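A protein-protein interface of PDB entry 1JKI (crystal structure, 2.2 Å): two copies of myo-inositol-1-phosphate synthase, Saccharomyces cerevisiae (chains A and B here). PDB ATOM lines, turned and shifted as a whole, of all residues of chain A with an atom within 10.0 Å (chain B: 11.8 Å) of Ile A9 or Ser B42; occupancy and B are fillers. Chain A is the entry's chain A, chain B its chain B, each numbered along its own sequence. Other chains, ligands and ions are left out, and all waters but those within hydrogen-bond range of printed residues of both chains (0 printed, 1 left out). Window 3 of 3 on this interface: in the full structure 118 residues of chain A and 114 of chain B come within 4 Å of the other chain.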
ATOM      1  N   ILE A   9      -2.775 -25.983   4.079  1.00  0.00           N
ATOM      2  CA  ILE A   9      -3.628 -26.942   3.276  1.00  0.00           C
ATOM      3  C   ILE A   9      -4.025 -26.443   1.864  1.00  0.00           C
ATOM      4  O   ILE A   9      -4.701 -25.426   1.740  1.00  0.00           O
ATOM      5  CB  ILE A   9      -4.914 -27.314   4.052  1.00  0.00           C
ATOM      6  CG1 ILE A   9      -4.526 -28.089   5.323  1.00  0.00           C
ATOM      7  CG2 ILE A   9      -5.865 -28.092   3.139  1.00  0.00           C
ATOM      8  CD1 ILE A   9      -3.450 -27.377   6.160  1.00  0.00           C
ATOM      9  N   THR A  10      -3.583 -27.182   0.829  1.00  0.00           N
ATOM     10  CA  THR A  10      -3.822 -26.875  -0.586  1.00  0.00           C
ATOM     11  C   THR A  10      -4.958 -27.709  -1.130  1.00  0.00           C
ATOM     12  O   THR A  10      -5.183 -28.865  -0.716  1.00  0.00           O
ATOM     13  CB  THR A  10      -2.544 -27.160  -1.506  1.00  0.00           C
ATOM     14  OG1 THR A  10      -1.504 -26.233  -1.167  1.00  0.00           O
ATOM     15  CG2 THR A  10      -2.862 -26.971  -3.012  1.00  0.00           C
ATOM     16  N   SER A  11      -5.695 -27.129  -2.058  1.00  0.00           N
ATOM     17  CA  SER A  11      -6.740 -27.938  -2.623  1.00  0.00           C
ATOM     18  C   SER A  11      -7.156 -27.430  -3.967  1.00  0.00           C
ATOM     19  O   SER A  11      -6.895 -26.287  -4.392  1.00  0.00           O
ATOM     20  CB  SER A  11      -7.964 -27.965  -1.688  1.00  0.00           C
ATOM     21  OG  SER A  11      -8.397 -26.617  -1.509  1.00  0.00           O
ATOM     22  N   VAL A  12      -7.885 -28.315  -4.627  1.00  0.00           N
ATOM     23  CA  VAL A  12      -8.381 -27.928  -5.930  1.00  0.00           C
ATOM     24  C   VAL A  12      -9.889 -28.147  -6.095  1.00  0.00           C
ATOM     25  O   VAL A  12     -10.467 -29.171  -5.694  1.00  0.00           O
ATOM     26  CB  VAL A  12      -7.461 -28.566  -7.164  1.00  0.00           C
ATOM     27  CG1 VAL A  12      -7.427 -29.994  -7.173  1.00  0.00           C
ATOM     28  CG2 VAL A  12      -7.966 -28.130  -8.468  1.00  0.00           C
ATOM     29  N   LYS A  13     -10.506 -27.145  -6.704  1.00  0.00           N
ATOM     30  CA  LYS A  13     -11.965 -27.187  -7.026  1.00  0.00           C
ATOM     31  C   LYS A  13     -12.237 -27.098  -8.574  1.00  0.00           C
ATOM     32  O   LYS A  13     -12.023 -26.017  -9.174  1.00  0.00           O
ATOM     33  CB  LYS A  13     -12.646 -25.994  -6.401  1.00  0.00           C
ATOM     34  CG  LYS A  13     -14.134 -26.045  -6.559  1.00  0.00           C
ATOM     35  CD  LYS A  13     -14.625 -27.346  -5.952  1.00  0.00           C
ATOM     36  CE  LYS A  13     -16.132 -27.379  -5.978  1.00  0.00           C
ATOM     37  NZ  LYS A  13     -16.458 -28.705  -6.719  1.00  0.00           N
ATOM     38  N   LYS A  62     -11.059 -40.310   4.183  1.00  0.00           N
ATOM     39  CA  LYS A  62      -9.886 -41.194   4.292  1.00  0.00           C
ATOM     40  C   LYS A  62      -9.661 -41.650   5.787  1.00  0.00           C
ATOM     41  O   LYS A  62      -9.986 -40.908   6.725  1.00  0.00           O
ATOM     42  CB  LYS A  62      -8.690 -40.489   3.702  1.00  0.00           C
ATOM     43  CG  LYS A  62      -8.453 -39.207   4.286  1.00  0.00           C
ATOM     44  CD  LYS A  62      -7.306 -38.448   3.633  1.00  0.00           C
ATOM     45  CE  LYS A  62      -7.128 -37.310   4.598  1.00  0.00           C
ATOM     46  NZ  LYS A  62      -6.184 -36.191   4.425  1.00  0.00           N
ATOM     47  N   PRO A 129       0.226 -29.755  -6.122  1.00  0.00           N
ATOM     48  CA  PRO A 129       0.780 -30.968  -5.530  1.00  0.00           C
ATOM     49  C   PRO A 129      -0.008 -32.153  -5.959  1.00  0.00           C
ATOM     50  O   PRO A 129      -1.222 -32.123  -6.005  1.00  0.00           O
ATOM     51  CB  PRO A 129       0.635 -30.747  -4.034  1.00  0.00           C
ATOM     52  CG  PRO A 129       0.867 -29.261  -3.890  1.00  0.00           C
ATOM     53  CD  PRO A 129       0.132 -28.651  -5.117  1.00  0.00           C
ATOM     54  N   ASN A 131      -0.697 -34.464  -4.391  1.00  0.00           N
ATOM     55  CA  ASN A 131      -1.611 -35.024  -3.505  1.00  0.00           C
ATOM     56  C   ASN A 131      -2.648 -34.027  -3.080  1.00  0.00           C
ATOM     57  O   ASN A 131      -3.302 -34.273  -2.105  1.00  0.00           O
ATOM     58  CB  ASN A 131      -0.928 -35.651  -2.324  1.00  0.00           C
ATOM     59  CG  ASN A 131      -0.269 -34.627  -1.415  1.00  0.00           C
ATOM     60  OD1 ASN A 131      -0.142 -33.489  -1.712  1.00  0.00           O
ATOM     61  ND2 ASN A 131       0.172 -35.105  -0.257  1.00  0.00           N
ATOM     62  N   SER A 132      -2.781 -32.914  -3.790  1.00  0.00           N
ATOM     63  CA  SER A 132      -3.749 -31.964  -3.442  1.00  0.00           C
ATOM     64  C   SER A 132      -5.082 -32.001  -4.304  1.00  0.00           C
ATOM     65  O   SER A 132      -5.957 -31.138  -4.107  1.00  0.00           O
ATOM     66  CB  SER A 132      -3.095 -30.604  -3.567  1.00  0.00           C
ATOM     67  OG  SER A 132      -2.801 -30.270  -4.955  1.00  0.00           O
ATOM     68  N   LEU A 133      -5.192 -32.936  -5.286  1.00  0.00           N
ATOM     69  CA  LEU A 133      -6.318 -32.999  -6.242  1.00  0.00           C
ATOM     70  C   LEU A 133      -7.513 -33.643  -5.513  1.00  0.00           C
ATOM     71  O   LEU A 133      -8.502 -33.010  -5.460  1.00  0.00           O
ATOM     72  CB  LEU A 133      -5.891 -33.788  -7.494  1.00  0.00           C
ATOM     73  CG  LEU A 133      -5.244 -33.023  -8.723  1.00  0.00           C
ATOM     74  CD1 LEU A 133      -3.879 -32.360  -8.283  1.00  0.00           C
ATOM     75  CD2 LEU A 133      -5.015 -34.045  -9.904  1.00  0.00           C
ATOM     76  N   PRO A 135      -8.370 -36.416  -1.817  1.00  0.00           N
ATOM     77  CA  PRO A 135      -7.905 -36.829  -0.485  1.00  0.00           C
ATOM     78  C   PRO A 135      -7.089 -38.014  -0.404  1.00  0.00           C
ATOM     79  O   PRO A 135      -7.488 -39.137  -0.739  1.00  0.00           O
ATOM     80  CB  PRO A 135      -9.235 -36.969   0.324  1.00  0.00           C
ATOM     81  CG  PRO A 135     -10.192 -37.732  -0.798  1.00  0.00           C
ATOM     82  CD  PRO A 135      -9.824 -36.716  -1.994  1.00  0.00           C
ATOM     83  N   THR B  38      -7.059 -20.386 -11.148  1.00  0.00           N
ATOM     84  CA  THR B  38      -6.689 -19.180 -10.397  1.00  0.00           C
ATOM     85  C   THR B  38      -6.295 -19.741  -9.045  1.00  0.00           C
ATOM     86  O   THR B  38      -6.629 -20.876  -8.735  1.00  0.00           O
ATOM     87  CB  THR B  38      -7.883 -18.109 -10.387  1.00  0.00           C
ATOM     88  OG1 THR B  38      -9.085 -18.620  -9.781  1.00  0.00           O
ATOM     89  CG2 THR B  38      -8.260 -17.774 -11.817  1.00  0.00           C
ATOM     90  N   LYS B  39      -5.495 -19.055  -8.268  1.00  0.00           N
ATOM     91  CA  LYS B  39      -5.163 -19.626  -6.920  1.00  0.00           C
ATOM     92  C   LYS B  39      -5.673 -18.620  -5.911  1.00  0.00           C
ATOM     93  O   LYS B  39      -5.533 -17.431  -6.109  1.00  0.00           O
ATOM     94  CB  LYS B  39      -3.630 -19.837  -6.732  1.00  0.00           C
ATOM     95  CG  LYS B  39      -3.162 -20.500  -5.383  1.00  0.00           C
ATOM     96  CD  LYS B  39      -1.905 -21.481  -5.486  1.00  0.00           C
ATOM     97  CE  LYS B  39      -0.483 -20.822  -5.684  1.00  0.00           C
ATOM     98  NZ  LYS B  39       0.794 -21.824  -5.914  1.00  0.00           N
ATOM     99  N   THR B  40      -6.304 -19.103  -4.846  1.00  0.00           N
ATOM    100  CA  THR B  40      -6.856 -18.231  -3.776  1.00  0.00           C
ATOM    101  C   THR B  40      -5.910 -17.339  -2.996  1.00  0.00           C
ATOM    102  O   THR B  40      -6.076 -16.101  -2.917  1.00  0.00           O
ATOM    103  CB  THR B  40      -7.443 -19.054  -2.677  1.00  0.00           C
ATOM    104  OG1 THR B  40      -6.637 -20.235  -2.554  1.00  0.00           O
ATOM    105  CG2 THR B  40      -8.869 -19.384  -2.945  1.00  0.00           C
ATOM    106  N   ALA B  41      -4.943 -18.005  -2.366  1.00  0.00           N
ATOM    107  CA  ALA B  41      -4.004 -17.384  -1.436  1.00  0.00           C
ATOM    108  C   ALA B  41      -4.522 -17.962  -0.093  1.00  0.00           C
ATOM    109  O   ALA B  41      -4.211 -17.440   0.974  1.00  0.00           O
ATOM    110  CB  ALA B  41      -4.092 -15.858  -1.432  1.00  0.00           C
ATOM    111  N   SER B  42      -5.369 -19.010  -0.172  1.00  0.00           N
ATOM    112  CA  SER B  42      -5.886 -19.796   1.016  1.00  0.00           C
ATOM    113  C   SER B  42      -5.523 -21.227   0.565  1.00  0.00           C
ATOM    114  O   SER B  42      -5.936 -22.256   1.179  1.00  0.00           O
ATOM    115  CB  SER B  42      -7.419 -19.690   1.229  1.00  0.00           C
ATOM    116  OG  SER B  42      -8.190 -20.161   0.098  1.00  0.00           O
ATOM    117  N   GLY B  43      -4.789 -21.272  -0.559  1.00  0.00           N
ATOM    118  CA  GLY B  43      -4.296 -22.526  -1.087  1.00  0.00           C
ATOM    119  C   GLY B  43      -5.189 -23.382  -1.948  1.00  0.00           C
ATOM    120  O   GLY B  43      -4.941 -24.650  -2.085  1.00  0.00           O
ATOM    121  N   ARG B  44      -6.196 -22.719  -2.544  1.00  0.00           N
ATOM    122  CA  ARG B  44      -7.133 -23.431  -3.409  1.00  0.00           C
ATOM    123  C   ARG B  44      -7.006 -23.068  -4.877  1.00  0.00           C
ATOM    124  O   ARG B  44      -6.884 -21.910  -5.265  1.00  0.00           O
ATOM    125  CB  ARG B  44      -8.582 -23.222  -2.965  1.00  0.00           C
ATOM    126  CG  ARG B  44      -9.564 -23.775  -3.971  1.00  0.00           C
ATOM    127  CD  ARG B  44     -10.972 -23.763  -3.398  1.00  0.00           C
ATOM    128  NE  ARG B  44     -11.833 -22.690  -3.913  1.00  0.00           N
ATOM    129  CZ  ARG B  44     -11.976 -21.446  -3.420  1.00  0.00           C
ATOM    130  NH1 ARG B  44     -11.317 -20.972  -2.356  1.00  0.00           N
ATOM    131  NH2 ARG B  44     -12.889 -20.672  -3.970  1.00  0.00           N
ATOM    132  N   PHE B  45      -7.008 -24.092  -5.697  1.00  0.00           N
ATOM    133  CA  PHE B  45      -6.925 -23.829  -7.110  1.00  0.00           C
ATOM    134  C   PHE B  45      -8.333 -23.977  -7.760  1.00  0.00           C
ATOM    135  O   PHE B  45      -8.908 -25.082  -7.818  1.00  0.00           O
ATOM    136  CB  PHE B  45      -5.958 -24.836  -7.804  1.00  0.00           C
ATOM    137  CG  PHE B  45      -4.512 -24.795  -7.333  1.00  0.00           C
ATOM    138  CD1 PHE B  45      -4.085 -25.575  -6.231  1.00  0.00           C
ATOM    139  CD2 PHE B  45      -3.556 -24.072  -8.065  1.00  0.00           C
ATOM    140  CE1 PHE B  45      -2.768 -25.641  -5.902  1.00  0.00           C
ATOM    141  CE2 PHE B  45      -2.197 -24.108  -7.753  1.00  0.00           C
ATOM    142  CZ  PHE B  45      -1.788 -24.883  -6.692  1.00  0.00           C
ATOM    143  N   ASP B  46      -8.884 -22.889  -8.278  1.00  0.00           N
ATOM    144  CA  ASP B  46     -10.189 -22.977  -8.966  1.00  0.00           C
ATOM    145  C   ASP B  46      -9.918 -23.224 -10.412  1.00  0.00           C
ATOM    146  O   ASP B  46      -9.165 -22.457 -11.088  1.00  0.00           O
ATOM    147  CB  ASP B  46     -10.954 -21.706  -8.777  1.00  0.00           C
ATOM    148  CG  ASP B  46     -11.346 -21.519  -7.330  1.00  0.00           C
ATOM    149  OD1 ASP B  46     -12.111 -22.335  -6.741  1.00  0.00           O
ATOM    150  OD2 ASP B  46     -10.812 -20.526  -6.814  1.00  0.00           O
ATOM    151  N   ASP B 385       6.907 -26.106  -6.617  1.00  0.00           N
ATOM    152  CA  ASP B 385       7.213 -25.289  -5.492  1.00  0.00           C
ATOM    153  C   ASP B 385       7.072 -26.137  -4.193  1.00  0.00           C
ATOM    154  O   ASP B 385       7.122 -25.610  -3.090  1.00  0.00           O
ATOM    155  CB  ASP B 385       6.351 -24.010  -5.536  1.00  0.00           C
ATOM    156  CG  ASP B 385       4.821 -24.280  -5.329  1.00  0.00           C
ATOM    157  OD1 ASP B 385       4.062 -23.269  -5.302  1.00  0.00           O
ATOM    158  OD2 ASP B 385       4.405 -25.464  -5.198  1.00  0.00           O
ATOM    159  N   ILE B 386       6.851 -27.449  -4.321  1.00  0.00           N
ATOM    160  CA  ILE B 386       6.870 -28.225  -3.094  1.00  0.00           C
ATOM    161  C   ILE B 386       8.394 -28.279  -2.758  1.00  0.00           C
ATOM    162  O   ILE B 386       8.837 -28.135  -1.609  1.00  0.00           O
ATOM    163  CB  ILE B 386       6.448 -29.691  -3.290  1.00  0.00           C
ATOM    164  CG1 ILE B 386       4.960 -29.799  -3.758  1.00  0.00           C
ATOM    165  CG2 ILE B 386       6.678 -30.450  -1.918  1.00  0.00           C
ATOM    166  CD1 ILE B 386       4.561 -31.208  -3.915  1.00  0.00           C
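No position is printed for both chains. Of the 11 pairs that touch across the chains among the printed residues, none has its exchanged pair printed and touching as well.
Of the 11 printed residues of chain A, 6 touch a printed residue of chain B. Hydrophobic or aromatic side chains of chain A within 4 Å of the printed part of chain B: Val A12 and Pro A129. Of the 11 printed residues of chain B, 6 touch a printed residue of chain A. Printed residues of chain B that touch a printed residue of chain A: Ser B42, Gly B43, Arg B44, Phe B45, Asp B46 and Ile B386. Hydrophobic or aromatic side chains of chain B that line the printed part of chain A: Phe B45 and Ile B386. Among the printed residues, 11 pairs touch across the chains. Among the printed residues, no Asp or Glu carboxylate lies within 4 Å of a Lys or Arg side-chain nitrogen of the other chain.
Of chain B, only Ser B42 (3.4 Å) and Gly B43 (3.9 Å) come within 4 Å of Ile A9. Of the printed residues of chain B, Thr A10 touches Gly B43 and Phe B45. Ser A11 touches just these residues of chain B: Gly B43 (2.6 Å), Arg B44 (3.0 Å) and Phe B45 (2.6 Å). Ser A132 touches none of the printed residues of chain B. Pro A135 touches none of the printed residues of chain B. No residue of chain A comes within 4 Å of Ala B41. Of chain A, only Ile A9 comes within 4 Å of Ser B42. Printed residues of chain A within 4 Å of Arg B44: Ser A11. Printed residues of chain A within 4 Å of Phe B45: Thr A10 (3.2 Å), Ser A11 (2.6 Å), Val A12 (3.3 Å) and Lys A13 (2.8 Å). The nearest residue of chain B that does not touch Ile A9 is Arg B44 (5.3 Å). The nearest residue of chain A that does not touch Ser B42 is Thr A10 (5.4 Å). The nearest printed residue of chain A that does not touch Arg B44 is Lys A13 (4.1 Å).
Among the printed residues, merely in contact across the chains: Thr A10 with Gly B43 (2.9 Å), Ser A11 with Arg B44 (3.0 Å), Thr A10 with Phe B45 (3.2 Å), Val A12 with Phe B45 (3.3 Å), Lys A13 with Asp B46 (3.6 Å), Ile A9 with Gly B43 (3.9 Å) and Pro A129 with Ile B386 (3.95 Å).
NE of Arg B44 lies within salt-bridge range of OD1 of Asp B46, at 2.9 Å. The side-chain hydroxyl (OG1) of Thr B40 is in hydrogen-bond range of the backbone NH (N) of Ser B42 (3.0 Å). The side-chain hydroxyl of Ser A132 is in hydrogen-bond range of the backbone carbonyl oxygen of Pro A129 (2.7 Å). N of Val A12 lies within hydrogen-bond range of O of Ser A132 (3.5 Å). OG1 of Thr B40 sits at hydrogen-bond distance from N of Gly B43 (2.9 Å). N of Arg B44 is in hydrogen-bond range of OG1 of Thr B40, at 2.5 Å.
O of Gly B43 is in hydrogen-bond range of N of Ser A11, 2.6 Å away. N of Phe B45 sits at hydrogen-bond distance from O of Ser A11 (2.6 Å). N of Lys A13 lies within hydrogen-bond range of O of Phe B45 (2.8 Å). O of Ser B42 sits close to O of Ile A9, at 3.4 Å.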
